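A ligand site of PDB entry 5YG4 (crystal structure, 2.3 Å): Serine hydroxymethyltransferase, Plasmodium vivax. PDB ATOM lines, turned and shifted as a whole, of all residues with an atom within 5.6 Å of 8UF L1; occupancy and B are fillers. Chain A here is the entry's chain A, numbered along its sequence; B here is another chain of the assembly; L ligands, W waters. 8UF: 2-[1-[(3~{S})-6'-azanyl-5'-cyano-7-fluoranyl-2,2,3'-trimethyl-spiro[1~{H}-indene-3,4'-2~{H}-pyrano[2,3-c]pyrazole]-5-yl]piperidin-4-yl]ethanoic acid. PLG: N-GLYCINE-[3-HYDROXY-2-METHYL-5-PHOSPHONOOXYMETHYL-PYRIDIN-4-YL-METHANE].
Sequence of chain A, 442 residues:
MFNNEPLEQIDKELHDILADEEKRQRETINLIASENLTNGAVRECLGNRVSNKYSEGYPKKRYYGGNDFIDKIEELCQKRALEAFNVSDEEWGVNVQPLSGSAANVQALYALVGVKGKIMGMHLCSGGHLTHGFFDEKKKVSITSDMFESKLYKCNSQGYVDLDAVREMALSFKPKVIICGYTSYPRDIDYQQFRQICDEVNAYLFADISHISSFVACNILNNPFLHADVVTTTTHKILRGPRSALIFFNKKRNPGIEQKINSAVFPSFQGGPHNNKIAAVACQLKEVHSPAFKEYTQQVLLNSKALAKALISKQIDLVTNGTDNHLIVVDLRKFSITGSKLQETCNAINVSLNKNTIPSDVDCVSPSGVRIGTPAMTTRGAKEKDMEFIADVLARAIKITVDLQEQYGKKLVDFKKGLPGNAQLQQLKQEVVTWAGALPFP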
ATOM      1  N   LEU A 124       6.158 -18.363 -13.569  1.00  0.00           N
ATOM      2  CA  LEU A 124       5.976 -17.201 -12.676  1.00  0.00           C
ATOM      3  C   LEU A 124       7.254 -16.550 -12.182  1.00  0.00           C
ATOM      4  O   LEU A 124       7.412 -15.348 -12.271  1.00  0.00           O
ATOM      5  CB  LEU A 124       5.154 -17.639 -11.479  1.00  0.00           C
ATOM      6  CG  LEU A 124       4.894 -16.684 -10.310  1.00  0.00           C
ATOM      7  CD1 LEU A 124       4.057 -15.515 -10.780  1.00  0.00           C
ATOM      8  CD2 LEU A 124       4.146 -17.436  -9.222  1.00  0.00           C
ATOM      9  N   CYS A 125       8.132 -17.358 -11.609  1.00  0.00           N
ATOM     10  CA  CYS A 125       9.491 -16.936 -11.203  1.00  0.00           C
ATOM     11  C   CYS A 125      10.359 -16.308 -12.264  1.00  0.00           C
ATOM     12  O   CYS A 125      11.198 -15.465 -11.948  1.00  0.00           O
ATOM     13  CB  CYS A 125      10.237 -18.089 -10.521  1.00  0.00           C
ATOM     14  SG  CYS A 125       9.505 -18.537  -8.915  1.00  0.00           S
ATOM     15  N   GLY A 127       9.099 -14.411 -14.748  1.00  0.00           N
ATOM     16  CA  GLY A 127       8.384 -13.236 -15.274  1.00  0.00           C
ATOM     17  C   GLY A 127       6.985 -13.496 -15.832  1.00  0.00           C
ATOM     18  O   GLY A 127       6.258 -12.552 -16.088  1.00  0.00           O
ATOM     19  N   GLY A 128       6.603 -14.760 -16.008  1.00  0.00           N
ATOM     20  CA  GLY A 128       5.253 -15.094 -16.469  1.00  0.00           C
ATOM     21  C   GLY A 128       4.161 -14.738 -15.471  1.00  0.00           C
ATOM     22  O   GLY A 128       4.436 -14.614 -14.268  1.00  0.00           O
ATOM     23  N   HIS A 129       2.949 -14.521 -15.989  1.00  0.00           N
ATOM     24  CA  HIS A 129       1.755 -14.316 -15.169  1.00  0.00           C
ATOM     25  C   HIS A 129       1.138 -15.638 -14.722  1.00  0.00           C
ATOM     26  O   HIS A 129       1.384 -16.685 -15.321  1.00  0.00           O
ATOM     27  CB  HIS A 129       0.688 -13.495 -15.915  1.00  0.00           C
ATOM     28  CG  HIS A 129      -0.334 -12.855 -15.019  1.00  0.00           C
ATOM     29  ND1 HIS A 129      -1.649 -13.262 -14.964  1.00  0.00           N
ATOM     30  CD2 HIS A 129      -0.204 -11.889 -14.075  1.00  0.00           C
ATOM     31  CE1 HIS A 129      -2.289 -12.549 -14.050  1.00  0.00           C
ATOM     32  NE2 HIS A 129      -1.427 -11.706 -13.496  1.00  0.00           N
ATOM     33  N   LEU A 130       0.323 -15.571 -13.675  1.00  0.00           N
ATOM     34  CA  LEU A 130      -0.415 -16.719 -13.155  1.00  0.00           C
ATOM     35  C   LEU A 130      -1.302 -17.361 -14.207  1.00  0.00           C
ATOM     36  O   LEU A 130      -1.404 -18.568 -14.261  1.00  0.00           O
ATOM     37  CB  LEU A 130      -1.280 -16.305 -11.954  1.00  0.00           C
ATOM     38  CG  LEU A 130      -0.566 -15.972 -10.629  1.00  0.00           C
ATOM     39  CD1 LEU A 130      -1.543 -15.383  -9.633  1.00  0.00           C
ATOM     40  CD2 LEU A 130       0.065 -17.213 -10.021  1.00  0.00           C
ATOM     41  N   PHE A 134       0.251 -21.164 -14.545  1.00  0.00           N
ATOM     42  CA  PHE A 134       1.062 -21.358 -13.354  1.00  0.00           C
ATOM     43  C   PHE A 134       0.549 -22.416 -12.386  1.00  0.00           C
ATOM     44  O   PHE A 134      -0.632 -22.403 -11.974  1.00  0.00           O
ATOM     45  CB  PHE A 134       1.324 -20.108 -12.538  1.00  0.00           C
ATOM     46  CG  PHE A 134       2.319 -20.354 -11.438  1.00  0.00           C
ATOM     47  CD1 PHE A 134       3.628 -20.689 -11.747  1.00  0.00           C
ATOM     48  CD2 PHE A 134       1.926 -20.386 -10.109  1.00  0.00           C
ATOM     49  CE1 PHE A 134       4.551 -20.974 -10.747  1.00  0.00           C
ATOM     50  CE2 PHE A 134       2.841 -20.685  -9.115  1.00  0.00           C
ATOM     51  CZ  PHE A 134       4.152 -20.968  -9.432  1.00  0.00           C
ATOM     52  N   ASP A 136       2.552 -25.037  -9.040  1.00  0.00           N
ATOM     53  CA  ASP A 136       3.729 -25.456  -8.308  1.00  0.00           C
ATOM     54  C   ASP A 136       3.590 -26.953  -8.008  1.00  0.00           C
ATOM     55  O   ASP A 136       2.551 -27.562  -8.292  1.00  0.00           O
ATOM     56  CB  ASP A 136       3.947 -24.606  -7.033  1.00  0.00           C
ATOM     57  CG  ASP A 136       2.880 -24.810  -5.948  1.00  0.00           C
ATOM     58  OD1 ASP A 136       1.988 -25.679  -6.065  1.00  0.00           O
ATOM     59  OD2 ASP A 136       2.946 -24.097  -4.936  1.00  0.00           O
ATOM     60  N   VAL A 141      -2.054 -23.758  -8.786  1.00  0.00           N
ATOM     61  CA  VAL A 141      -2.314 -22.396  -8.320  1.00  0.00           C
ATOM     62  C   VAL A 141      -3.325 -21.643  -9.228  1.00  0.00           C
ATOM     63  O   VAL A 141      -4.295 -21.048  -8.740  1.00  0.00           O
ATOM     64  CB  VAL A 141      -0.974 -21.613  -8.172  1.00  0.00           C
ATOM     65  CG1 VAL A 141      -1.194 -20.138  -7.927  1.00  0.00           C
ATOM     66  CG2 VAL A 141      -0.127 -22.208  -7.049  1.00  0.00           C
ATOM     67  N   THR A 183       4.672 -10.445 -17.093  1.00  0.00           N
ATOM     68  CA  THR A 183       4.328  -9.524 -15.983  1.00  0.00           C
ATOM     69  C   THR A 183       5.544  -8.809 -15.412  1.00  0.00           C
ATOM     70  O   THR A 183       5.431  -7.649 -15.070  1.00  0.00           O
ATOM     71  CB  THR A 183       3.518 -10.152 -14.831  1.00  0.00           C
ATOM     72  OG1 THR A 183       4.282 -10.120 -13.600  1.00  0.00           O
ATOM     73  CG2 THR A 183       3.118 -11.473 -15.116  1.00  0.00           C
ATOM     74  N   SER A 184       6.692  -9.489 -15.357  1.00  0.00           N
ATOM     75  CA  SER A 184       7.952  -8.916 -14.834  1.00  0.00           C
ATOM     76  C   SER A 184       9.158  -9.181 -15.727  1.00  0.00           C
ATOM     77  O   SER A 184      10.230  -9.469 -15.228  1.00  0.00           O
ATOM     78  CB  SER A 184       8.253  -9.509 -13.452  1.00  0.00           C
ATOM     79  OG  SER A 184       7.083  -9.510 -12.669  1.00  0.00           O
ATOM     80  N   ASN A 354       6.862  -3.723  -5.432  1.00  0.00           N
ATOM     81  CA  ASN A 354       6.555  -5.076  -5.009  1.00  0.00           C
ATOM     82  C   ASN A 354       7.776  -5.941  -5.038  1.00  0.00           C
ATOM     83  O   ASN A 354       8.711  -5.731  -5.837  1.00  0.00           O
ATOM     84  CB  ASN A 354       5.413  -5.688  -5.839  1.00  0.00           C
ATOM     85  CG  ASN A 354       5.714  -5.749  -7.313  1.00  0.00           C
ATOM     86  OD1 ASN A 354       5.504  -4.772  -8.059  1.00  0.00           O
ATOM     87  ND2 ASN A 354       6.222  -6.882  -7.757  1.00  0.00           N
ATOM     88  N   LYS A 355       7.777  -6.907  -4.133  1.00  0.00           N
ATOM     89  CA  LYS A 355       8.756  -7.978  -4.127  1.00  0.00           C
ATOM     90  C   LYS A 355       8.582  -8.793  -5.412  1.00  0.00           C
ATOM     91  O   LYS A 355       7.515  -8.838  -5.988  1.00  0.00           O
ATOM     92  CB  LYS A 355       8.622  -8.868  -2.898  1.00  0.00           C
ATOM     93  CG  LYS A 355       7.201  -9.362  -2.584  1.00  0.00           C
ATOM     94  CD  LYS A 355       7.176 -10.604  -1.737  1.00  0.00           C
ATOM     95  CE  LYS A 355       5.750 -11.103  -1.572  1.00  0.00           C
ATOM     96  NZ  LYS A 355       5.576 -11.757  -0.254  1.00  0.00           N
ATOM     97  N   ASN A 356       9.667  -9.415  -5.847  1.00  0.00           N
ATOM     98  CA  ASN A 356       9.704 -10.087  -7.123  1.00  0.00           C
ATOM     99  C   ASN A 356      10.803 -11.147  -7.132  1.00  0.00           C
ATOM    100  O   ASN A 356      11.947 -10.906  -6.720  1.00  0.00           O
ATOM    101  CB  ASN A 356       9.929  -9.086  -8.268  1.00  0.00           C
ATOM    102  CG  ASN A 356       9.253  -9.540  -9.555  1.00  0.00           C
ATOM    103  OD1 ASN A 356       8.158  -9.080  -9.886  1.00  0.00           O
ATOM    104  ND2 ASN A 356       9.844 -10.522 -10.199  1.00  0.00           N
ATOM    105  N   THR A 357      10.438 -12.323  -7.642  1.00  0.00           N
ATOM    106  CA  THR A 357      11.379 -13.419  -7.877  1.00  0.00           C
ATOM    107  C   THR A 357      12.445 -13.030  -8.903  1.00  0.00           C
ATOM    108  O   THR A 357      12.200 -12.194  -9.772  1.00  0.00           O
ATOM    109  CB  THR A 357      10.629 -14.659  -8.409  1.00  0.00           C
ATOM    110  OG1 THR A 357       9.786 -14.280  -9.502  1.00  0.00           O
ATOM    111  CG2 THR A 357       9.771 -15.294  -7.312  1.00  0.00           C
ATOM    112  N   CYS A 364       8.577 -18.832  -4.570  1.00  0.00           N
ATOM    113  CA  CYS A 364       7.981 -17.495  -4.566  1.00  0.00           C
ATOM    114  C   CYS A 364       7.809 -16.817  -3.197  1.00  0.00           C
ATOM    115  O   CYS A 364       7.506 -15.615  -3.147  1.00  0.00           O
ATOM    116  CB  CYS A 364       6.614 -17.556  -5.208  1.00  0.00           C
ATOM    117  SG  CYS A 364       6.563 -18.088  -6.922  1.00  0.00           S
ATOM    118  N   VAL A 365       7.912 -17.574  -2.104  1.00  0.00           N
ATOM    119  CA  VAL A 365       7.985 -16.972  -0.769  1.00  0.00           C
ATOM    120  C   VAL A 365       9.456 -16.719  -0.502  1.00  0.00           C
ATOM    121  O   VAL A 365      10.292 -17.606  -0.720  1.00  0.00           O
ATOM    122  CB  VAL A 365       7.352 -17.873   0.311  1.00  0.00           C
ATOM    123  CG1 VAL A 365       7.789 -17.470   1.723  1.00  0.00           C
ATOM    124  CG2 VAL A 365       5.828 -17.816   0.190  1.00  0.00           C
ATOM    125  N   PRO A 367      11.221 -14.072  -2.164  1.00  0.00           N
ATOM    126  CA  PRO A 367      11.950 -13.746  -3.391  1.00  0.00           C
ATOM    127  C   PRO A 367      13.082 -12.747  -3.172  1.00  0.00           C
ATOM    128  O   PRO A 367      13.058 -11.967  -2.204  1.00  0.00           O
ATOM    129  CB  PRO A 367      10.881 -13.139  -4.292  1.00  0.00           C
ATOM    130  CG  PRO A 367       9.835 -12.668  -3.376  1.00  0.00           C
ATOM    131  CD  PRO A 367       9.834 -13.615  -2.231  1.00  0.00           C
ATOM    132  N   ARG A 371      10.484  -5.342  -8.001  1.00  0.00           N
ATOM    133  CA  ARG A 371      10.181  -4.816  -9.304  1.00  0.00           C
ATOM    134  C   ARG A 371       9.745  -3.361  -9.169  1.00  0.00           C
ATOM    135  O   ARG A 371       8.954  -3.028  -8.285  1.00  0.00           O
ATOM    136  CB  ARG A 371       9.088  -5.653  -9.925  1.00  0.00           C
ATOM    137  CG  ARG A 371       8.797  -5.366 -11.372  1.00  0.00           C
ATOM    138  CD  ARG A 371       7.500  -6.045 -11.793  1.00  0.00           C
ATOM    139  NE  ARG A 371       6.299  -5.429 -11.194  1.00  0.00           N
ATOM    140  CZ  ARG A 371       5.059  -5.875 -11.376  1.00  0.00           C
ATOM    141  NH1 ARG A 371       4.825  -6.929 -12.146  1.00  0.00           N
ATOM    142  NH2 ARG A 371       4.042  -5.269 -10.789  1.00  0.00           N
ATOM    143  N   GLU B  56      -3.858  -7.399  -4.966  1.00  0.00           N
ATOM    144  CA  GLU B  56      -4.052  -8.846  -5.045  1.00  0.00           C
ATOM    145  C   GLU B  56      -3.881  -9.507  -3.702  1.00  0.00           C
ATOM    146  O   GLU B  56      -3.002  -9.141  -2.933  1.00  0.00           O
ATOM    147  CB  GLU B  56      -3.055  -9.448  -6.000  1.00  0.00           C
ATOM    148  CG  GLU B  56      -3.321  -9.002  -7.409  1.00  0.00           C
ATOM    149  CD  GLU B  56      -2.397  -9.646  -8.388  1.00  0.00           C
ATOM    150  OE1 GLU B  56      -1.196  -9.383  -8.301  1.00  0.00           O
ATOM    151  OE2 GLU B  56      -2.890 -10.394  -9.223  1.00  0.00           O
ATOM    152  N   TYR B  63      -0.362  -9.180  -1.114  1.00  0.00           N
ATOM    153  CA  TYR B  63       0.944  -9.434  -1.712  1.00  0.00           C
ATOM    154  C   TYR B  63       1.737  -8.151  -1.804  1.00  0.00           C
ATOM    155  O   TYR B  63       2.958  -8.155  -1.657  1.00  0.00           O
ATOM    156  CB  TYR B  63       0.807 -10.074  -3.092  1.00  0.00           C
ATOM    157  CG  TYR B  63       0.395 -11.525  -3.017  1.00  0.00           C
ATOM    158  CD1 TYR B  63      -0.916 -11.887  -2.711  1.00  0.00           C
ATOM    159  CD2 TYR B  63       1.312 -12.541  -3.232  1.00  0.00           C
ATOM    160  CE1 TYR B  63      -1.298 -13.208  -2.619  1.00  0.00           C
ATOM    161  CE2 TYR B  63       0.942 -13.876  -3.154  1.00  0.00           C
ATOM    162  CZ  TYR B  63      -0.373 -14.207  -2.850  1.00  0.00           C
ATOM    163  OH  TYR B  63      -0.774 -15.538  -2.778  1.00  0.00           O
ATOM    164  N   TYR B  64       1.015  -7.053  -2.054  1.00  0.00           N
ATOM    165  CA  TYR B  64       1.595  -5.709  -2.105  1.00  0.00           C
ATOM    166  C   TYR B  64       1.245  -4.977  -0.837  1.00  0.00           C
ATOM    167  O   TYR B  64       0.318  -5.345  -0.139  1.00  0.00           O
ATOM    168  CB  TYR B  64       0.990  -4.904  -3.252  1.00  0.00           C
ATOM    169  CG  TYR B  64       1.362  -5.369  -4.620  1.00  0.00           C
ATOM    170  CD1 TYR B  64       2.117  -6.521  -4.819  1.00  0.00           C
ATOM    171  CD2 TYR B  64       0.948  -4.632  -5.734  1.00  0.00           C
ATOM    172  CE1 TYR B  64       2.446  -6.929  -6.083  1.00  0.00           C
ATOM    173  CE2 TYR B  64       1.288  -5.036  -7.020  1.00  0.00           C
ATOM    174  CZ  TYR B  64       2.043  -6.190  -7.197  1.00  0.00           C
ATOM    175  OH  TYR B  64       2.386  -6.625  -8.450  1.00  0.00           O
ATOM    176  N   PHE B 266      -9.171 -15.887  -5.974  1.00  0.00           N
ATOM    177  CA  PHE B 266      -7.772 -15.576  -6.274  1.00  0.00           C
ATOM    178  C   PHE B 266      -6.880 -16.514  -5.489  1.00  0.00           C
ATOM    179  O   PHE B 266      -7.099 -16.663  -4.303  1.00  0.00           O
ATOM    180  CB  PHE B 266      -7.456 -14.134  -5.870  1.00  0.00           C
ATOM    181  CG  PHE B 266      -5.990 -13.776  -5.967  1.00  0.00           C
ATOM    182  CD1 PHE B 266      -5.126 -14.016  -4.914  1.00  0.00           C
ATOM    183  CD2 PHE B 266      -5.475 -13.195  -7.129  1.00  0.00           C
ATOM    184  CE1 PHE B 266      -3.789 -13.674  -5.005  1.00  0.00           C
ATOM    185  CE2 PHE B 266      -4.148 -12.858  -7.230  1.00  0.00           C
ATOM    186  CZ  PHE B 266      -3.294 -13.100  -6.177  1.00  0.00           C
ATOM    187  N   PRO B 267      -5.820 -17.075  -6.089  1.00  0.00           N
ATOM    188  CA  PRO B 267      -5.323 -16.731  -7.431  1.00  0.00           C
ATOM    189  C   PRO B 267      -5.784 -17.618  -8.575  1.00  0.00           C
ATOM    190  O   PRO B 267      -5.297 -17.444  -9.714  1.00  0.00           O
ATOM    191  CB  PRO B 267      -3.797 -16.805  -7.271  1.00  0.00           C
ATOM    192  CG  PRO B 267      -3.519 -17.381  -5.919  1.00  0.00           C
ATOM    193  CD  PRO B 267      -4.803 -17.782  -5.284  1.00  0.00           C
HETATM  194  C2  8UF L   1       4.681 -12.485 -11.329  1.00  0.00           C
HETATM  195  C3  8UF L   1       4.810 -12.302  -9.979  1.00  0.00           C
HETATM  196  C4  8UF L   1       3.591 -11.875  -9.139  1.00  0.00           C
HETATM  197  C5  8UF L   1       2.308 -12.270  -9.806  1.00  0.00           C
HETATM  198  C6  8UF L   1       2.243 -12.521 -11.242  1.00  0.00           C
HETATM  199  N7  8UF L   1       5.665 -12.838 -12.145  1.00  0.00           N
HETATM  200  C8  8UF L   1       5.954 -12.418  -9.399  1.00  0.00           C
HETATM  201  C10 8UF L   1       0.876 -12.524  -9.403  1.00  0.00           C
HETATM  202  C13 8UF L   1       0.174 -12.470  -8.049  1.00  0.00           C
HETATM  203  C15 8UF L   1       2.367  -9.656  -8.456  1.00  0.00           C
HETATM  204  C16 8UF L   1       3.621 -12.539  -7.809  1.00  0.00           C
HETATM  205  C17 8UF L   1       4.167 -11.704  -6.883  1.00  0.00           C
HETATM  206  C18 8UF L   1       4.308 -12.102  -5.580  1.00  0.00           C
HETATM  207  C20 8UF L   1       3.197 -13.838  -7.482  1.00  0.00           C
HETATM  208  O54 8UF L   1       0.902 -19.818  -2.418  1.00  0.00           O
HETATM  209  C52 8UF L   1       0.251 -19.574  -3.485  1.00  0.00           C
HETATM  210  O53 8UF L   1      -1.022 -19.583  -3.536  1.00  0.00           O
HETATM  211  C51 8UF L   1       1.070 -19.303  -4.747  1.00  0.00           C
HETATM  212  C38 8UF L   1       1.638 -17.868  -4.865  1.00  0.00           C
HETATM  213  C37 8UF L   1       3.154 -17.839  -4.907  1.00  0.00           C
HETATM  214  C36 8UF L   1       3.629 -16.368  -4.843  1.00  0.00           C
HETATM  215  C39 8UF L   1       1.106 -17.247  -6.119  1.00  0.00           C
HETATM  216  C40 8UF L   1       1.398 -15.759  -6.111  1.00  0.00           C
HETATM  217  N35 8UF L   1       2.819 -15.537  -5.741  1.00  0.00           N
HETATM  218  C19 8UF L   1       3.325 -14.285  -6.160  1.00  0.00           C
HETATM  219  C41 8UF L   1       3.882 -13.390  -5.225  1.00  0.00           C
HETATM  220  F29 8UF L   1       4.854 -11.250  -4.694  1.00  0.00           F
HETATM  221  C44 8UF L   1       4.565 -10.375  -7.482  1.00  0.00           C
HETATM  222  C14 8UF L   1       3.712 -10.347  -8.775  1.00  0.00           C
HETATM  223  C30 8UF L   1       4.408  -9.460  -9.833  1.00  0.00           C
HETATM  224  N9  8UF L   1       7.007 -12.528  -8.883  1.00  0.00           N
HETATM  225  N11 8UF L   1       0.236 -12.847 -10.564  1.00  0.00           N
HETATM  226  N12 8UF L   1       1.048 -12.875 -11.702  1.00  0.00           N
HETATM  227  O1  8UF L   1       3.376 -12.363 -11.970  1.00  0.00           O
HETATM  228  N1  PLG L   2      -1.338 -10.320 -17.873  1.00  0.00           N
HETATM  229  C2  PLG L   2      -0.172  -9.840 -17.443  1.00  0.00           C
HETATM  230  C2A PLG L   2       1.062 -10.031 -18.296  1.00  0.00           C
HETATM  231  C3  PLG L   2      -0.141  -9.153 -16.154  1.00  0.00           C
HETATM  232  O3  PLG L   2       1.026  -8.679 -15.711  1.00  0.00           O
HETATM  233  C4  PLG L   2      -1.374  -9.016 -15.355  1.00  0.00           C
HETATM  234  C4A PLG L   2      -1.372  -8.285 -14.000  1.00  0.00           C
HETATM  235  C5  PLG L   2      -2.608  -9.602 -15.977  1.00  0.00           C
HETATM  236  C6  PLG L   2      -2.487 -10.239 -17.195  1.00  0.00           C
HETATM  237  C5A PLG L   2      -3.968  -9.651 -15.355  1.00  0.00           C
HETATM  238  OP4 PLG L   2      -4.587  -8.424 -15.043  1.00  0.00           O
HETATM  239  P   PLG L   2      -5.832  -8.453 -14.030  1.00  0.00           P
HETATM  240  OP1 PLG L   2      -6.555  -9.757 -14.127  1.00  0.00           O
HETATM  241  OP2 PLG L   2      -5.161  -8.296 -12.696  1.00  0.00           O
HETATM  242  OP3 PLG L   2      -6.557  -7.228 -14.479  1.00  0.00           O
HETATM  243  C   PLG L   2       0.839  -7.114 -11.706  1.00  0.00           C
HETATM  244  O   PLG L   2       0.724  -6.248 -10.843  1.00  0.00           O
HETATM  245  OXT PLG L   2       1.824  -7.097 -12.490  1.00  0.00           O
HETATM  246  CA  PLG L   2      -0.280  -8.174 -11.728  1.00  0.00           C
HETATM  247  N   PLG L   2      -0.407  -8.759 -13.053  1.00  0.00           N
HETATM  248  O   HOH W   1       3.527 -19.242  -1.232  1.00  0.00           O
HETATM  249  O   HOH W   2       7.265 -12.922  -5.636  1.00  0.00           O
HETATM  250  O   HOH W   3      -2.454 -12.604 -10.639  1.00  0.00           O
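Water W3 lies within hydrogen-bond range of the side-chain carboxylate of Glu 56 of chain B (2.7 Å), a nitrogen (N11) of 8UF L1 (2.7 Å) and a ring nitrogen (NE2) of His 129 (3.2 Å).
Merely in contact with 8UF L1: Gly 127 (3.97 Å), Val 141 (3.9 Å), Ser 184 (3.7 Å), Asn 354 (3.8 Å), Lys 355 (3.3 Å), Asn 356 (3.7 Å), Cys 364 (3.2 Å), Arg 371 (3.5 Å), Glu 56 of chain B (3.4 Å), Tyr 63 of chain B (3.4 Å), Tyr 64 of chain B (3.0 Å) and Phe 266 of chain B (3.99 Å). Of the 24 residues printed, 18 come within 4 Å of 8UF L1. The nearest printed residue that does not touch 8UF L1 is Pro 267 of chain B (4.1 Å).
A nitrogen (N9) of 8UF L1 sits at hydrogen-bond distance from the side-chain hydroxyl of Thr 357, 3.3 Å away. A ring nitrogen (NE2) of His 129 lies close to a nitrogen (N12) of 8UF L1 (3.3 Å). N of Leu 130 lies within hydrogen-bond range of N12 of 8UF L1 (3.4 Å). A ring nitrogen (NE2) of His 129 lies within hydrogen-bond range of a nitrogen (N) of PLG L2, at 3.1 Å. An oxygen (OXT) of PLG L2 is in salt-bridge range of the guanidinium group (NH1) of Arg 371 (3.0 Å). A nitrogen (N7) of 8UF L1 is in hydrogen-bond range of the backbone carbonyl oxygen (O) of Leu 124 (3.1 Å). OH of Tyr 64 of chain B lies within hydrogen-bond range of O of PLG L2, at 2.9 Å. The side-chain hydroxyl (OG1) of Thr 183 lies within hydrogen-bond range of an oxygen (O1) of 8UF L1, 2.9 Å away. The backbone carbonyl oxygen (O) of Gly 128 sits at hydrogen-bond distance from a nitrogen (N7) of 8UF L1 (3.0 Å).
OD1 of Asn 356 sits at hydrogen-bond distance from OG of Ser 184, 3.0 Å away. The backbone carbonyl oxygen (O) of Thr 183 lies within hydrogen-bond range of the guanidinium group (NH1) of Arg 371, 3.1 Å away. The backbone carbonyl oxygen (O) of Glu 56 of chain B lies within hydrogen-bond range of the backbone NH (N) of Tyr 63 of chain B (3.2 Å). The side-chain hydroxyl (OG1) of Thr 357 lies within hydrogen-bond range of the backbone carbonyl oxygen (O) of Cys 125, at 3.1 Å. NH2 of Arg 371 lies within hydrogen-bond range of OH of Tyr 64 of chain B. The guanidinium group (NH1) of Arg 371 is in hydrogen-bond range of the side-chain hydroxyl (OG) of Ser 184 (3.5 Å). The backbone NH (N) of Arg 371 sits at hydrogen-bond distance from the backbone carbonyl oxygen (O) of Asn 354 (2.8 Å). The side-chain sulfur (SG) of Cys 125 sits at hydrogen-bond distance from the side-chain sulfur (SG) of Cys 364 (3.6 Å).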
